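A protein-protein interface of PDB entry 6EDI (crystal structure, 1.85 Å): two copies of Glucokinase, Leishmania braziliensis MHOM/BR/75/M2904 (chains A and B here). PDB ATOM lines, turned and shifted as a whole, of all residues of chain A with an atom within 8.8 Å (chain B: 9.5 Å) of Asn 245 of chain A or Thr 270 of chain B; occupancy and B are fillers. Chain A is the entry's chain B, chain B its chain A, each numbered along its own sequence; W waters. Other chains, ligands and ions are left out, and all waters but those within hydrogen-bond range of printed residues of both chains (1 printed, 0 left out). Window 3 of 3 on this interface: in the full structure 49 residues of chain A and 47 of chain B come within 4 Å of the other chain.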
ATOM      1  N   SER A 241      21.709  21.597 -15.017  1.00  0.00           N
ATOM      2  CA  SER A 241      21.259  22.570 -16.008  1.00  0.00           C
ATOM      3  C   SER A 241      19.750  22.546 -16.168  1.00  0.00           C
ATOM      4  O   SER A 241      19.109  21.503 -15.955  1.00  0.00           O
ATOM      5  CB  SER A 241      21.938  22.288 -17.344  1.00  0.00           C
ATOM      6  OG  SER A 241      23.256  22.821 -17.326  1.00  0.00           O
ATOM      7  N   TRP A 242      19.186  23.695 -16.542  1.00  0.00           N
ATOM      8  CA  TRP A 242      17.773  23.786 -16.904  1.00  0.00           C
ATOM      9  C   TRP A 242      17.430  22.890 -18.087  1.00  0.00           C
ATOM     10  O   TRP A 242      18.212  22.729 -19.011  1.00  0.00           O
ATOM     11  CB  TRP A 242      17.399  25.233 -17.254  1.00  0.00           C
ATOM     12  CG  TRP A 242      15.919  25.417 -17.454  1.00  0.00           C
ATOM     13  CD1 TRP A 242      14.992  25.741 -16.496  1.00  0.00           C
ATOM     14  CD2 TRP A 242      15.197  25.295 -18.685  1.00  0.00           C
ATOM     15  NE1 TRP A 242      13.736  25.818 -17.064  1.00  0.00           N
ATOM     16  CE2 TRP A 242      13.836  25.538 -18.402  1.00  0.00           C
ATOM     17  CE3 TRP A 242      15.566  24.983 -19.999  1.00  0.00           C
ATOM     18  CZ2 TRP A 242      12.844  25.498 -19.393  1.00  0.00           C
ATOM     19  CZ3 TRP A 242      14.575  24.931 -20.982  1.00  0.00           C
ATOM     20  CH2 TRP A 242      13.235  25.193 -20.670  1.00  0.00           C
ATOM     21  N   CYS A 243      16.248  22.291 -18.042  1.00  0.00           N
ATOM     22  CA  CYS A 243      15.779  21.451 -19.131  1.00  0.00           C
ATOM     23  C   CYS A 243      14.274  21.426 -19.023  1.00  0.00           C
ATOM     24  O   CYS A 243      13.710  21.962 -18.061  1.00  0.00           O
ATOM     25  CB  CYS A 243      16.348  20.043 -19.017  1.00  0.00           C
ATOM     26  SG  CYS A 243      16.148  19.315 -17.369  1.00  0.00           S
ATOM     27  N   ALA A 244      13.622  20.812 -20.004  1.00  0.00           N
ATOM     28  CA  ALA A 244      12.166  20.784 -20.020  1.00  0.00           C
ATOM     29  C   ALA A 244      11.647  19.361 -20.167  1.00  0.00           C
ATOM     30  O   ALA A 244      12.412  18.395 -20.122  1.00  0.00           O
ATOM     31  CB  ALA A 244      11.632  21.651 -21.129  1.00  0.00           C
ATOM     32  N   ASN A 245      10.332  19.247 -20.319  1.00  0.00           N
ATOM     33  CA  ASN A 245       9.697  17.976 -20.634  1.00  0.00           C
ATOM     34  C   ASN A 245      10.089  16.843 -19.659  1.00  0.00           C
ATOM     35  O   ASN A 245      10.116  17.069 -18.453  1.00  0.00           O
ATOM     36  CB  ASN A 245       9.969  17.652 -22.108  1.00  0.00           C
ATOM     37  CG  ASN A 245       9.479  18.773 -23.037  1.00  0.00           C
ATOM     38  OD1 ASN A 245       8.324  19.172 -22.962  1.00  0.00           O
ATOM     39  ND2 ASN A 245      10.373  19.327 -23.856  1.00  0.00           N
ATOM     40  N   GLU A 246      10.400  15.654 -20.173  1.00  0.00           N
ATOM     41  CA  GLU A 246      10.670  14.493 -19.314  1.00  0.00           C
ATOM     42  C   GLU A 246      11.947  14.664 -18.490  1.00  0.00           C
ATOM     43  O   GLU A 246      12.034  14.193 -17.345  1.00  0.00           O
ATOM     44  CB  GLU A 246      10.741  13.206 -20.142  1.00  0.00           C
ATOM     45  CG  GLU A 246       9.449  12.857 -20.890  1.00  0.00           C
ATOM     46  CD  GLU A 246       8.359  12.299 -19.978  1.00  0.00           C
ATOM     47  OE1 GLU A 246       8.343  11.066 -19.754  1.00  0.00           O
ATOM     48  OE2 GLU A 246       7.518  13.089 -19.486  1.00  0.00           O
ATOM     49  N   ASP A 247      12.933  15.334 -19.077  1.00  0.00           N
ATOM     50  CA  ASP A 247      14.180  15.615 -18.380  1.00  0.00           C
ATOM     51  C   ASP A 247      13.947  16.478 -17.130  1.00  0.00           C
ATOM     52  O   ASP A 247      14.499  16.190 -16.067  1.00  0.00           O
ATOM     53  CB  ASP A 247      15.193  16.265 -19.327  1.00  0.00           C
ATOM     54  CG  ASP A 247      15.749  15.290 -20.350  1.00  0.00           C
ATOM     55  OD1 ASP A 247      15.732  14.074 -20.096  1.00  0.00           O
ATOM     56  OD2 ASP A 247      16.214  15.732 -21.413  1.00  0.00           O
ATOM     57  N   SER A 248      13.125  17.524 -17.258  1.00  0.00           N
ATOM     58  CA  SER A 248      12.789  18.382 -16.115  1.00  0.00           C
ATOM     59  C   SER A 248      11.993  17.619 -15.066  1.00  0.00           C
ATOM     60  O   SER A 248      12.113  17.908 -13.877  1.00  0.00           O
ATOM     61  CB  SER A 248      12.017  19.632 -16.543  1.00  0.00           C
ATOM     62  OG  SER A 248      11.711  20.437 -15.412  1.00  0.00           O
ATOM     63  N   LYS A 249      11.181  16.657 -15.513  1.00  0.00           N
ATOM     64  CA  LYS A 249      10.463  15.757 -14.607  1.00  0.00           C
ATOM     65  C   LYS A 249      11.424  14.967 -13.715  1.00  0.00           C
ATOM     66  O   LYS A 249      11.185  14.808 -12.518  1.00  0.00           O
ATOM     67  CB  LYS A 249       9.614  14.762 -15.401  1.00  0.00           C
ATOM     68  CG  LYS A 249       8.581  15.383 -16.298  1.00  0.00           C
ATOM     69  CD  LYS A 249       7.608  16.223 -15.506  1.00  0.00           C
ATOM     70  CE  LYS A 249       6.641  16.933 -16.449  1.00  0.00           C
ATOM     71  NZ  LYS A 249       5.978  15.940 -17.347  1.00  0.00           N
ATOM     72  N   TYR A 250      12.506  14.473 -14.305  1.00  0.00           N
ATOM     73  CA  TYR A 250      13.528  13.758 -13.538  1.00  0.00           C
ATOM     74  C   TYR A 250      14.279  14.685 -12.582  1.00  0.00           C
ATOM     75  O   TYR A 250      14.518  14.326 -11.420  1.00  0.00           O
ATOM     76  CB  TYR A 250      14.534  13.038 -14.447  1.00  0.00           C
ATOM     77  CG  TYR A 250      15.739  12.554 -13.669  1.00  0.00           C
ATOM     78  CD1 TYR A 250      15.670  11.398 -12.903  1.00  0.00           C
ATOM     79  CD2 TYR A 250      16.933  13.273 -13.670  1.00  0.00           C
ATOM     80  CE1 TYR A 250      16.758  10.954 -12.170  1.00  0.00           C
ATOM     81  CE2 TYR A 250      18.024  12.841 -12.934  1.00  0.00           C
ATOM     82  CZ  TYR A 250      17.932  11.679 -12.191  1.00  0.00           C
ATOM     83  OH  TYR A 250      19.019  11.239 -11.453  1.00  0.00           O
ATOM     84  N   VAL A 251      14.670  15.862 -13.070  1.00  0.00           N
ATOM     85  CA  VAL A 251      15.384  16.814 -12.211  1.00  0.00           C
ATOM     86  C   VAL A 251      14.517  17.181 -11.007  1.00  0.00           C
ATOM     87  O   VAL A 251      15.002  17.287  -9.891  1.00  0.00           O
ATOM     88  CB  VAL A 251      15.810  18.110 -12.955  1.00  0.00           C
ATOM     89  CG1 VAL A 251      16.517  19.048 -11.989  1.00  0.00           C
ATOM     90  CG2 VAL A 251      16.726  17.784 -14.126  1.00  0.00           C
ATOM     91  N   GLN A 252      13.222  17.361 -11.244  1.00  0.00           N
ATOM     92  CA  GLN A 252      12.279  17.720 -10.185  1.00  0.00           C
ATOM     93  C   GLN A 252      12.130  16.590  -9.155  1.00  0.00           C
ATOM     94  O   GLN A 252      12.107  16.833  -7.934  1.00  0.00           O
ATOM     95  CB  GLN A 252      10.925  18.098 -10.818  1.00  0.00           C
ATOM     96  CG  GLN A 252       9.820  18.464  -9.829  1.00  0.00           C
ATOM     97  CD  GLN A 252       9.960  19.884  -9.311  1.00  0.00           C
ATOM     98  OE1 GLN A 252       9.117  20.755  -9.554  1.00  0.00           O
ATOM     99  NE2 GLN A 252      11.037  20.122  -8.592  1.00  0.00           N
ATOM    100  N   TYR A 290      13.482   5.249  -9.817  1.00  0.00           N
ATOM    101  CA  TYR A 290      12.792   6.106 -10.776  1.00  0.00           C
ATOM    102  C   TYR A 290      12.315   5.344 -12.003  1.00  0.00           C
ATOM    103  O   TYR A 290      11.193   5.530 -12.453  1.00  0.00           O
ATOM    104  CB  TYR A 290      13.711   7.254 -11.207  1.00  0.00           C
ATOM    105  CG  TYR A 290      12.983   8.349 -11.985  1.00  0.00           C
ATOM    106  CD1 TYR A 290      12.212   9.296 -11.324  1.00  0.00           C
ATOM    107  CD2 TYR A 290      13.072   8.427 -13.370  1.00  0.00           C
ATOM    108  CE1 TYR A 290      11.545  10.303 -12.021  1.00  0.00           C
ATOM    109  CE2 TYR A 290      12.396   9.425 -14.081  1.00  0.00           C
ATOM    110  CZ  TYR A 290      11.639  10.360 -13.393  1.00  0.00           C
ATOM    111  OH  TYR A 290      10.976  11.365 -14.077  1.00  0.00           O
ATOM    112  N   ARG A 325      20.985   6.623 -17.697  1.00  0.00           N
ATOM    113  CA  ARG A 325      20.693   7.975 -17.230  1.00  0.00           C
ATOM    114  C   ARG A 325      21.858   8.554 -16.440  1.00  0.00           C
ATOM    115  O   ARG A 325      22.167   9.737 -16.563  1.00  0.00           O
ATOM    116  CB  ARG A 325      19.429   8.014 -16.363  1.00  0.00           C
ATOM    117  CG  ARG A 325      18.945   9.442 -16.108  1.00  0.00           C
ATOM    118  CD  ARG A 325      17.822   9.485 -15.091  1.00  0.00           C
ATOM    119  NE  ARG A 325      16.589   8.834 -15.546  1.00  0.00           N
ATOM    120  CZ  ARG A 325      15.652   9.428 -16.287  1.00  0.00           C
ATOM    121  NH1 ARG A 325      15.810  10.683 -16.676  1.00  0.00           N
ATOM    122  NH2 ARG A 325      14.552   8.766 -16.651  1.00  0.00           N
ATOM    123  N   GLU A 375      24.218  18.078 -27.127  1.00  0.00           N
ATOM    124  CA  GLU A 375      22.942  18.757 -26.924  1.00  0.00           C
ATOM    125  C   GLU A 375      23.120  20.168 -26.373  1.00  0.00           C
ATOM    126  O   GLU A 375      22.198  20.998 -26.454  1.00  0.00           O
ATOM    127  CB  GLU A 375      22.031  17.945 -26.003  1.00  0.00           C
ATOM    128  CG  GLU A 375      21.666  16.571 -26.563  1.00  0.00           C
ATOM    129  CD  GLU A 375      20.652  15.834 -25.709  1.00  0.00           C
ATOM    130  OE1 GLU A 375      20.171  16.403 -24.702  1.00  0.00           O
ATOM    131  OE2 GLU A 375      20.338  14.679 -26.054  1.00  0.00           O
ATOM    132  N   ALA A 377      23.723  23.972 -25.785  1.00  0.00           N
ATOM    133  CA  ALA A 377      23.430  25.093 -26.695  1.00  0.00           C
ATOM    134  C   ALA A 377      24.667  25.555 -27.444  1.00  0.00           C
ATOM    135  O   ALA A 377      24.576  26.027 -28.580  1.00  0.00           O
ATOM    136  CB  ALA A 377      22.831  26.253 -25.936  1.00  0.00           C
ATOM    137  N   ARG A 380      25.479  22.982 -30.363  1.00  0.00           N
ATOM    138  CA  ARG A 380      24.478  23.106 -31.411  1.00  0.00           C
ATOM    139  C   ARG A 380      24.788  24.322 -32.269  1.00  0.00           C
ATOM    140  O   ARG A 380      24.760  24.249 -33.494  1.00  0.00           O
ATOM    141  CB  ARG A 380      23.085  23.224 -30.791  1.00  0.00           C
ATOM    142  CG  ARG A 380      22.620  21.946 -30.105  1.00  0.00           C
ATOM    143  CD  ARG A 380      21.346  22.171 -29.317  1.00  0.00           C
ATOM    144  NE  ARG A 380      20.850  20.928 -28.732  1.00  0.00           N
ATOM    145  CZ  ARG A 380      19.898  20.176 -29.276  1.00  0.00           C
ATOM    146  NH1 ARG A 380      19.335  20.539 -30.423  1.00  0.00           N
ATOM    147  NH2 ARG A 380      19.503  19.064 -28.672  1.00  0.00           N
ATOM    148  N   SER B 239      25.245  26.795 -19.166  1.00  0.00           N
ATOM    149  CA  SER B 239      23.780  26.754 -19.181  1.00  0.00           C
ATOM    150  C   SER B 239      23.172  27.303 -17.895  1.00  0.00           C
ATOM    151  O   SER B 239      23.716  27.093 -16.813  1.00  0.00           O
ATOM    152  CB  SER B 239      23.289  25.325 -19.380  1.00  0.00           C
ATOM    153  OG  SER B 239      23.862  24.750 -20.521  1.00  0.00           O
ATOM    154  N   MET B 240      22.040  28.003 -18.001  1.00  0.00           N
ATOM    155  CA  MET B 240      21.312  28.410 -16.801  1.00  0.00           C
ATOM    156  C   MET B 240      20.907  27.197 -15.960  1.00  0.00           C
ATOM    157  O   MET B 240      20.669  26.113 -16.489  1.00  0.00           O
ATOM    158  CB  MET B 240      20.079  29.253 -17.148  1.00  0.00           C
ATOM    159  CG  MET B 240      20.431  30.614 -17.701  1.00  0.00           C
ATOM    160  SD  MET B 240      18.987  31.647 -17.978  1.00  0.00           S
ATOM    161  CE  MET B 240      18.574  32.099 -16.292  1.00  0.00           C
ATOM    162  N   TRP B 242      18.788  24.704 -13.431  1.00  0.00           N
ATOM    163  CA  TRP B 242      17.410  24.267 -13.384  1.00  0.00           C
ATOM    164  C   TRP B 242      16.629  25.053 -12.327  1.00  0.00           C
ATOM    165  O   TRP B 242      17.187  25.502 -11.324  1.00  0.00           O
ATOM    166  CB  TRP B 242      17.344  22.751 -13.122  1.00  0.00           C
ATOM    167  CG  TRP B 242      15.962  22.218 -13.185  1.00  0.00           C
ATOM    168  CD1 TRP B 242      15.317  21.700 -14.275  1.00  0.00           C
ATOM    169  CD2 TRP B 242      15.044  22.150 -12.099  1.00  0.00           C
ATOM    170  NE1 TRP B 242      14.036  21.317 -13.921  1.00  0.00           N
ATOM    171  CE2 TRP B 242      13.851  21.582 -12.587  1.00  0.00           C
ATOM    172  CE3 TRP B 242      15.116  22.518 -10.750  1.00  0.00           C
ATOM    173  CZ2 TRP B 242      12.744  21.372 -11.774  1.00  0.00           C
ATOM    174  CZ3 TRP B 242      14.017  22.311  -9.947  1.00  0.00           C
ATOM    175  CH2 TRP B 242      12.843  21.748 -10.462  1.00  0.00           C
ATOM    176  N   SER B 248      11.350  29.314 -13.774  1.00  0.00           N
ATOM    177  CA  SER B 248      11.430  28.425 -14.936  1.00  0.00           C
ATOM    178  C   SER B 248      10.681  28.973 -16.159  1.00  0.00           C
ATOM    179  O   SER B 248      11.116  28.783 -17.295  1.00  0.00           O
ATOM    180  CB  SER B 248      10.934  27.016 -14.575  1.00  0.00           C
ATOM    181  OG  SER B 248      11.032  26.139 -15.676  1.00  0.00           O
ATOM    182  N   VAL B 251      13.162  31.245 -17.813  1.00  0.00           N
ATOM    183  CA  VAL B 251      14.210  30.552 -18.541  1.00  0.00           C
ATOM    184  C   VAL B 251      13.630  29.995 -19.827  1.00  0.00           C
ATOM    185  O   VAL B 251      14.251  30.062 -20.895  1.00  0.00           O
ATOM    186  CB  VAL B 251      14.862  29.419 -17.708  1.00  0.00           C
ATOM    187  CG1 VAL B 251      15.951  28.744 -18.523  1.00  0.00           C
ATOM    188  CG2 VAL B 251      15.433  29.962 -16.381  1.00  0.00           C
ATOM    189  N   GLN B 252      12.421  29.449 -19.718  1.00  0.00           N
ATOM    190  CA  GLN B 252      11.716  28.929 -20.884  1.00  0.00           C
ATOM    191  C   GLN B 252      11.547  29.998 -21.963  1.00  0.00           C
ATOM    192  O   GLN B 252      11.814  29.765 -23.154  1.00  0.00           O
ATOM    193  CB  GLN B 252      10.331  28.411 -20.485  1.00  0.00           C
ATOM    194  CG  GLN B 252       9.560  27.814 -21.665  1.00  0.00           C
ATOM    195  CD  GLN B 252      10.299  26.653 -22.312  1.00  0.00           C
ATOM    196  OE1 GLN B 252      10.200  25.504 -21.864  1.00  0.00           O
ATOM    197  NE2 GLN B 252      11.049  26.946 -23.361  1.00  0.00           N
ATOM    198  N   ALA B 253      11.085  31.170 -21.547  1.00  0.00           N
ATOM    199  CA  ALA B 253      10.841  32.244 -22.509  1.00  0.00           C
ATOM    200  C   ALA B 253      12.155  32.710 -23.117  1.00  0.00           C
ATOM    201  O   ALA B 253      12.221  33.017 -24.311  1.00  0.00           O
ATOM    202  CB  ALA B 253      10.097  33.400 -21.857  1.00  0.00           C
ATOM    203  N   LEU B 254      13.204  32.763 -22.293  1.00  0.00           N
ATOM    204  CA  LEU B 254      14.523  33.186 -22.775  1.00  0.00           C
ATOM    205  C   LEU B 254      15.047  32.201 -23.819  1.00  0.00           C
ATOM    206  O   LEU B 254      15.546  32.597 -24.864  1.00  0.00           O
ATOM    207  CB  LEU B 254      15.521  33.331 -21.611  1.00  0.00           C
ATOM    208  CG  LEU B 254      16.919  33.808 -22.010  1.00  0.00           C
ATOM    209  CD1 LEU B 254      16.813  35.173 -22.701  1.00  0.00           C
ATOM    210  CD2 LEU B 254      17.873  33.877 -20.810  1.00  0.00           C
ATOM    211  N   ALA B 255      14.896  30.916 -23.527  1.00  0.00           N
ATOM    212  CA  ALA B 255      15.324  29.840 -24.417  1.00  0.00           C
ATOM    213  C   ALA B 255      14.641  29.919 -25.785  1.00  0.00           C
ATOM    214  O   ALA B 255      15.294  29.795 -26.829  1.00  0.00           O
ATOM    215  CB  ALA B 255      15.028  28.496 -23.769  1.00  0.00           C
ATOM    216  N   GLY B 256      13.326  30.090 -25.770  1.00  0.00           N
ATOM    217  CA  GLY B 256      12.560  30.195 -27.004  1.00  0.00           C
ATOM    218  C   GLY B 256      12.936  31.433 -27.787  1.00  0.00           C
ATOM    219  O   GLY B 256      13.027  31.414 -29.022  1.00  0.00           O
ATOM    220  N   TYR B 257      13.157  32.523 -27.059  1.00  0.00           N
ATOM    221  CA  TYR B 257      13.621  33.771 -27.657  1.00  0.00           C
ATOM    222  C   TYR B 257      14.976  33.592 -28.323  1.00  0.00           C
ATOM    223  O   TYR B 257      15.176  34.026 -29.445  1.00  0.00           O
ATOM    224  CB  TYR B 257      13.696  34.851 -26.584  1.00  0.00           C
ATOM    225  CG  TYR B 257      14.172  36.213 -27.068  1.00  0.00           C
ATOM    226  CD1 TYR B 257      13.374  37.001 -27.892  1.00  0.00           C
ATOM    227  CD2 TYR B 257      15.396  36.724 -26.660  1.00  0.00           C
ATOM    228  CE1 TYR B 257      13.789  38.249 -28.317  1.00  0.00           C
ATOM    229  CE2 TYR B 257      15.828  37.975 -27.081  1.00  0.00           C
ATOM    230  CZ  TYR B 257      15.017  38.730 -27.916  1.00  0.00           C
ATOM    231  OH  TYR B 257      15.431  39.975 -28.336  1.00  0.00           O
ATOM    232  N   MET B 258      15.914  32.957 -27.623  1.00  0.00           N
ATOM    233  CA  MET B 258      17.250  32.727 -28.170  1.00  0.00           C
ATOM    234  C   MET B 258      17.237  31.803 -29.389  1.00  0.00           C
ATOM    235  O   MET B 258      18.120  31.867 -30.239  1.00  0.00           O
ATOM    236  CB  MET B 258      18.178  32.162 -27.088  1.00  0.00           C
ATOM    237  CG  MET B 258      18.524  33.141 -25.986  1.00  0.00           C
ATOM    238  SD  MET B 258      19.644  34.438 -26.568  1.00  0.00           S
ATOM    239  CE  MET B 258      18.517  35.767 -26.886  1.00  0.00           C
ATOM    240  N   ALA B 259      16.245  30.929 -29.476  1.00  0.00           N
ATOM    241  CA  ALA B 259      16.115  30.093 -30.670  1.00  0.00           C
ATOM    242  C   ALA B 259      15.485  30.876 -31.826  1.00  0.00           C
ATOM    243  O   ALA B 259      15.746  30.587 -32.997  1.00  0.00           O
ATOM    244  CB  ALA B 259      15.317  28.836 -30.371  1.00  0.00           C
ATOM    245  N   GLY B 266      20.347  23.839 -34.532  1.00  0.00           N
ATOM    246  CA  GLY B 266      19.313  22.992 -33.954  1.00  0.00           C
ATOM    247  C   GLY B 266      18.908  23.422 -32.554  1.00  0.00           C
ATOM    248  O   GLY B 266      18.757  22.595 -31.650  1.00  0.00           O
ATOM    249  N   LEU B 267      18.720  24.729 -32.393  1.00  0.00           N
ATOM    250  CA  LEU B 267      18.387  25.339 -31.121  1.00  0.00           C
ATOM    251  C   LEU B 267      16.882  25.273 -30.864  1.00  0.00           C
ATOM    252  O   LEU B 267      16.086  25.784 -31.653  1.00  0.00           O
ATOM    253  CB  LEU B 267      18.873  26.785 -31.123  1.00  0.00           C
ATOM    254  CG  LEU B 267      19.618  27.343 -29.911  1.00  0.00           C
ATOM    255  CD1 LEU B 267      18.685  28.175 -29.037  1.00  0.00           C
ATOM    256  CD2 LEU B 267      20.259  26.224 -29.097  1.00  0.00           C
ATOM    257  N   ASP B 268      16.506  24.616 -29.769  1.00  0.00           N
ATOM    258  CA  ASP B 268      15.113  24.495 -29.364  1.00  0.00           C
ATOM    259  C   ASP B 268      14.819  25.455 -28.233  1.00  0.00           C
ATOM    260  O   ASP B 268      15.724  26.097 -27.696  1.00  0.00           O
ATOM    261  CB  ASP B 268      14.826  23.076 -28.842  1.00  0.00           C
ATOM    262  CG  ASP B 268      14.615  22.074 -29.947  1.00  0.00           C
ATOM    263  OD1 ASP B 268      13.625  22.232 -30.697  1.00  0.00           O
ATOM    264  OD2 ASP B 268      15.424  21.121 -30.047  1.00  0.00           O
ATOM    265  N   SER B 269      13.549  25.531 -27.856  1.00  0.00           N
ATOM    266  CA  SER B 269      13.190  26.156 -26.601  1.00  0.00           C
ATOM    267  C   SER B 269      13.351  25.114 -25.492  1.00  0.00           C
ATOM    268  O   SER B 269      13.201  25.429 -24.308  1.00  0.00           O
ATOM    269  CB  SER B 269      11.758  26.693 -26.641  1.00  0.00           C
ATOM    270  OG  SER B 269      10.809  25.646 -26.697  1.00  0.00           O
ATOM    271  N   THR B 270      13.664  23.874 -25.872  1.00  0.00           N
ATOM    272  CA  THR B 270      13.935  22.828 -24.869  1.00  0.00           C
ATOM    273  C   THR B 270      15.391  22.842 -24.419  1.00  0.00           C
ATOM    274  O   THR B 270      15.746  22.160 -23.460  1.00  0.00           O
ATOM    275  CB  THR B 270      13.569  21.398 -25.347  1.00  0.00           C
ATOM    276  OG1 THR B 270      14.547  20.924 -26.286  1.00  0.00           O
ATOM    277  CG2 THR B 270      12.169  21.365 -25.970  1.00  0.00           C
ATOM    278  N   VAL B 271      16.217  23.619 -25.118  1.00  0.00           N
ATOM    279  CA  VAL B 271      17.637  23.756 -24.789  1.00  0.00           C
ATOM    280  C   VAL B 271      17.855  24.944 -23.847  1.00  0.00           C
ATOM    281  O   VAL B 271      17.459  26.055 -24.180  1.00  0.00           O
ATOM    282  CB  VAL B 271      18.467  24.022 -26.059  1.00  0.00           C
ATOM    283  CG1 VAL B 271      19.959  23.942 -25.751  1.00  0.00           C
ATOM    284  CG2 VAL B 271      18.100  23.049 -27.180  1.00  0.00           C
ATOM    285  N   ALA B 272      18.506  24.721 -22.699  1.00  0.00           N
ATOM    286  CA  ALA B 272      18.796  25.800 -21.741  1.00  0.00           C
ATOM    287  C   ALA B 272      19.551  26.946 -22.411  1.00  0.00           C
ATOM    288  O   ALA B 272      20.418  26.706 -23.254  1.00  0.00           O
ATOM    289  CB  ALA B 272      19.584  25.277 -20.564  1.00  0.00           C
ATOM    290  N   PRO B 273      19.205  28.195 -22.069  1.00  0.00           N
ATOM    291  CA  PRO B 273      19.995  29.293 -22.636  1.00  0.00           C
ATOM    292  C   PRO B 273      21.202  29.481 -21.744  1.00  0.00           C
ATOM    293  O   PRO B 273      21.168  28.986 -20.619  1.00  0.00           O
ATOM    294  CB  PRO B 273      19.053  30.493 -22.537  1.00  0.00           C
ATOM    295  CG  PRO B 273      18.167  30.195 -21.356  1.00  0.00           C
ATOM    296  CD  PRO B 273      18.090  28.674 -21.229  1.00  0.00           C
HETATM  297  O   HOH W   1      22.392  24.513 -22.810  1.00  0.00           O
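Of the 21 printed residues of chain B, 12 touch a printed residue of chain A.
Hydrophobic or aromatic side chains of chain B that line the printed part of chain A: Trp 242, Val 251, Val 271 and Ala 272.
Of the 17 printed residues of chain A, 10 touch a printed residue of chain B.
Hydrophobic or aromatic side chains of chain A within 4 Å of the printed part of chain B: Trp 242, Val 251 and Ala 377.
Among the printed residues, Asp or Glu carboxylates within 4 Å of a Lys or Arg side-chain nitrogen of the other chain: Arg 380 of chain A with Asp 268 of chain B (3.97 Å).
Met 240 of chain B touches Ser 241 of chain A (O to CA, 3.6 Å).
Trp 242 of chain A touches Val 251 of chain B (CG to CG1, 3.5 Å).
Trp 242 of chain A touches Ser 269 of chain B.
Ala 272 of chain B touches Trp 242 of chain A (CB to O, 3.3 Å).
Cys 243 of chain A touches Trp 242 of chain B (N to CD1, 3.9 Å).
Val 251 of chain A touches Trp 242 of chain B.
Gln 252 of chain A touches Trp 242 of chain B.
O of Glu 375 of chain A touches CG1 of Val 271 of chain B, 3.8 Å away.
Ala 272 of chain B touches Ala 377 of chain A (O to CB, 3.6 Å).
Arg 380 of chain A touches Val 271 of chain B (NE to CG2, 3.8 Å).
Trp 242 of chain B touches its own counterpart, Trp 242 of chain A.
Trp 242 of chain A touches Ser 248 of chain B, and with the chains exchanged Ser 248 of chain A touches Trp 242 of chain B.
Trp 242 of chain A touches Val 251 of chain B, and with the chains exchanged Val 251 of chain A touches Trp 242 of chain B.
Trp 242 of chain A touches Gln 252 of chain B, and with the chains exchanged Gln 252 of chain A touches Trp 242 of chain B.
Positions printed for both chains: 242, 248, 251 and 252.
O of Met 240 of chain B lies within hydrogen-bond range of N of Trp 242 of chain A.
NE1 of Trp 242 of chain B sits at hydrogen-bond distance from OG of Ser 248 of chain A, at 2.9 Å.
NE1 of Trp 242 of chain A sits at hydrogen-bond distance from OG of Ser 248 of chain B, 3.1 Å away.
O of Gly 266 of chain B is in hydrogen-bond range of NH1 of Arg 380 of chain A (2.5 Å).
NH1 of Arg 380 of chain A lies within salt-bridge range of OD2 of Asp 268 of chain B, 3.97 Å away.
N of Trp 242 of chain B lies close to N of Trp 242 of chain A (3.3 Å).
Printed residues of chain B within 4 Å of Glu 375 of chain A: Val 271 (3.8 Å).
Ala 253 of chain B touches none of the printed residues of chain A.
Of chain A, only Trp 242 (3.6 Å) comes within 4 Å of Ser 269 of chain B.
Thr 270 of chain B touches just these residues of chain A: Trp 242 and Asn 245.
Of the printed residues of chain A, Val 271 of chain B touches Glu 375, Ala 377 and Arg 380.
The nearest residue of chain A that does not touch Thr 270 of chain B is Ala 244 of chain A (4.3 Å).
The nearest printed residue of chain A that does not touch Ser 239 of chain B is Trp 242 of chain A (5.2 Å).
Water W1 lies within hydrogen-bond range of the side-chain hydroxyl of Ser 239 of chain B (2.7 Å), the backbone carbonyl oxygen of Ala 272 of chain B (3.0 Å) and the backbone NH of Ala 377 of chain A (3.3 Å).
The backbone NH of Met 240 of chain B is in hydrogen-bond range of the backbone carbonyl oxygen of Pro 273 of chain B (2.9 Å).
NE2 of Gln 252 of chain B is in hydrogen-bond range of O of Ser 269 of chain B, at 2.8 Å.
SG of Cys 243 of chain A sits close to O of Asp 247 of chain A.
SG of Cys 243 of chain A is in hydrogen-bond range of N of Ser 248 of chain A (3.5 Å).
The backbone carbonyl oxygen (O) of Glu 375 of chain A is in hydrogen-bond range of the guanidinium group (NE) of Arg 380 of chain A (2.6 Å).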
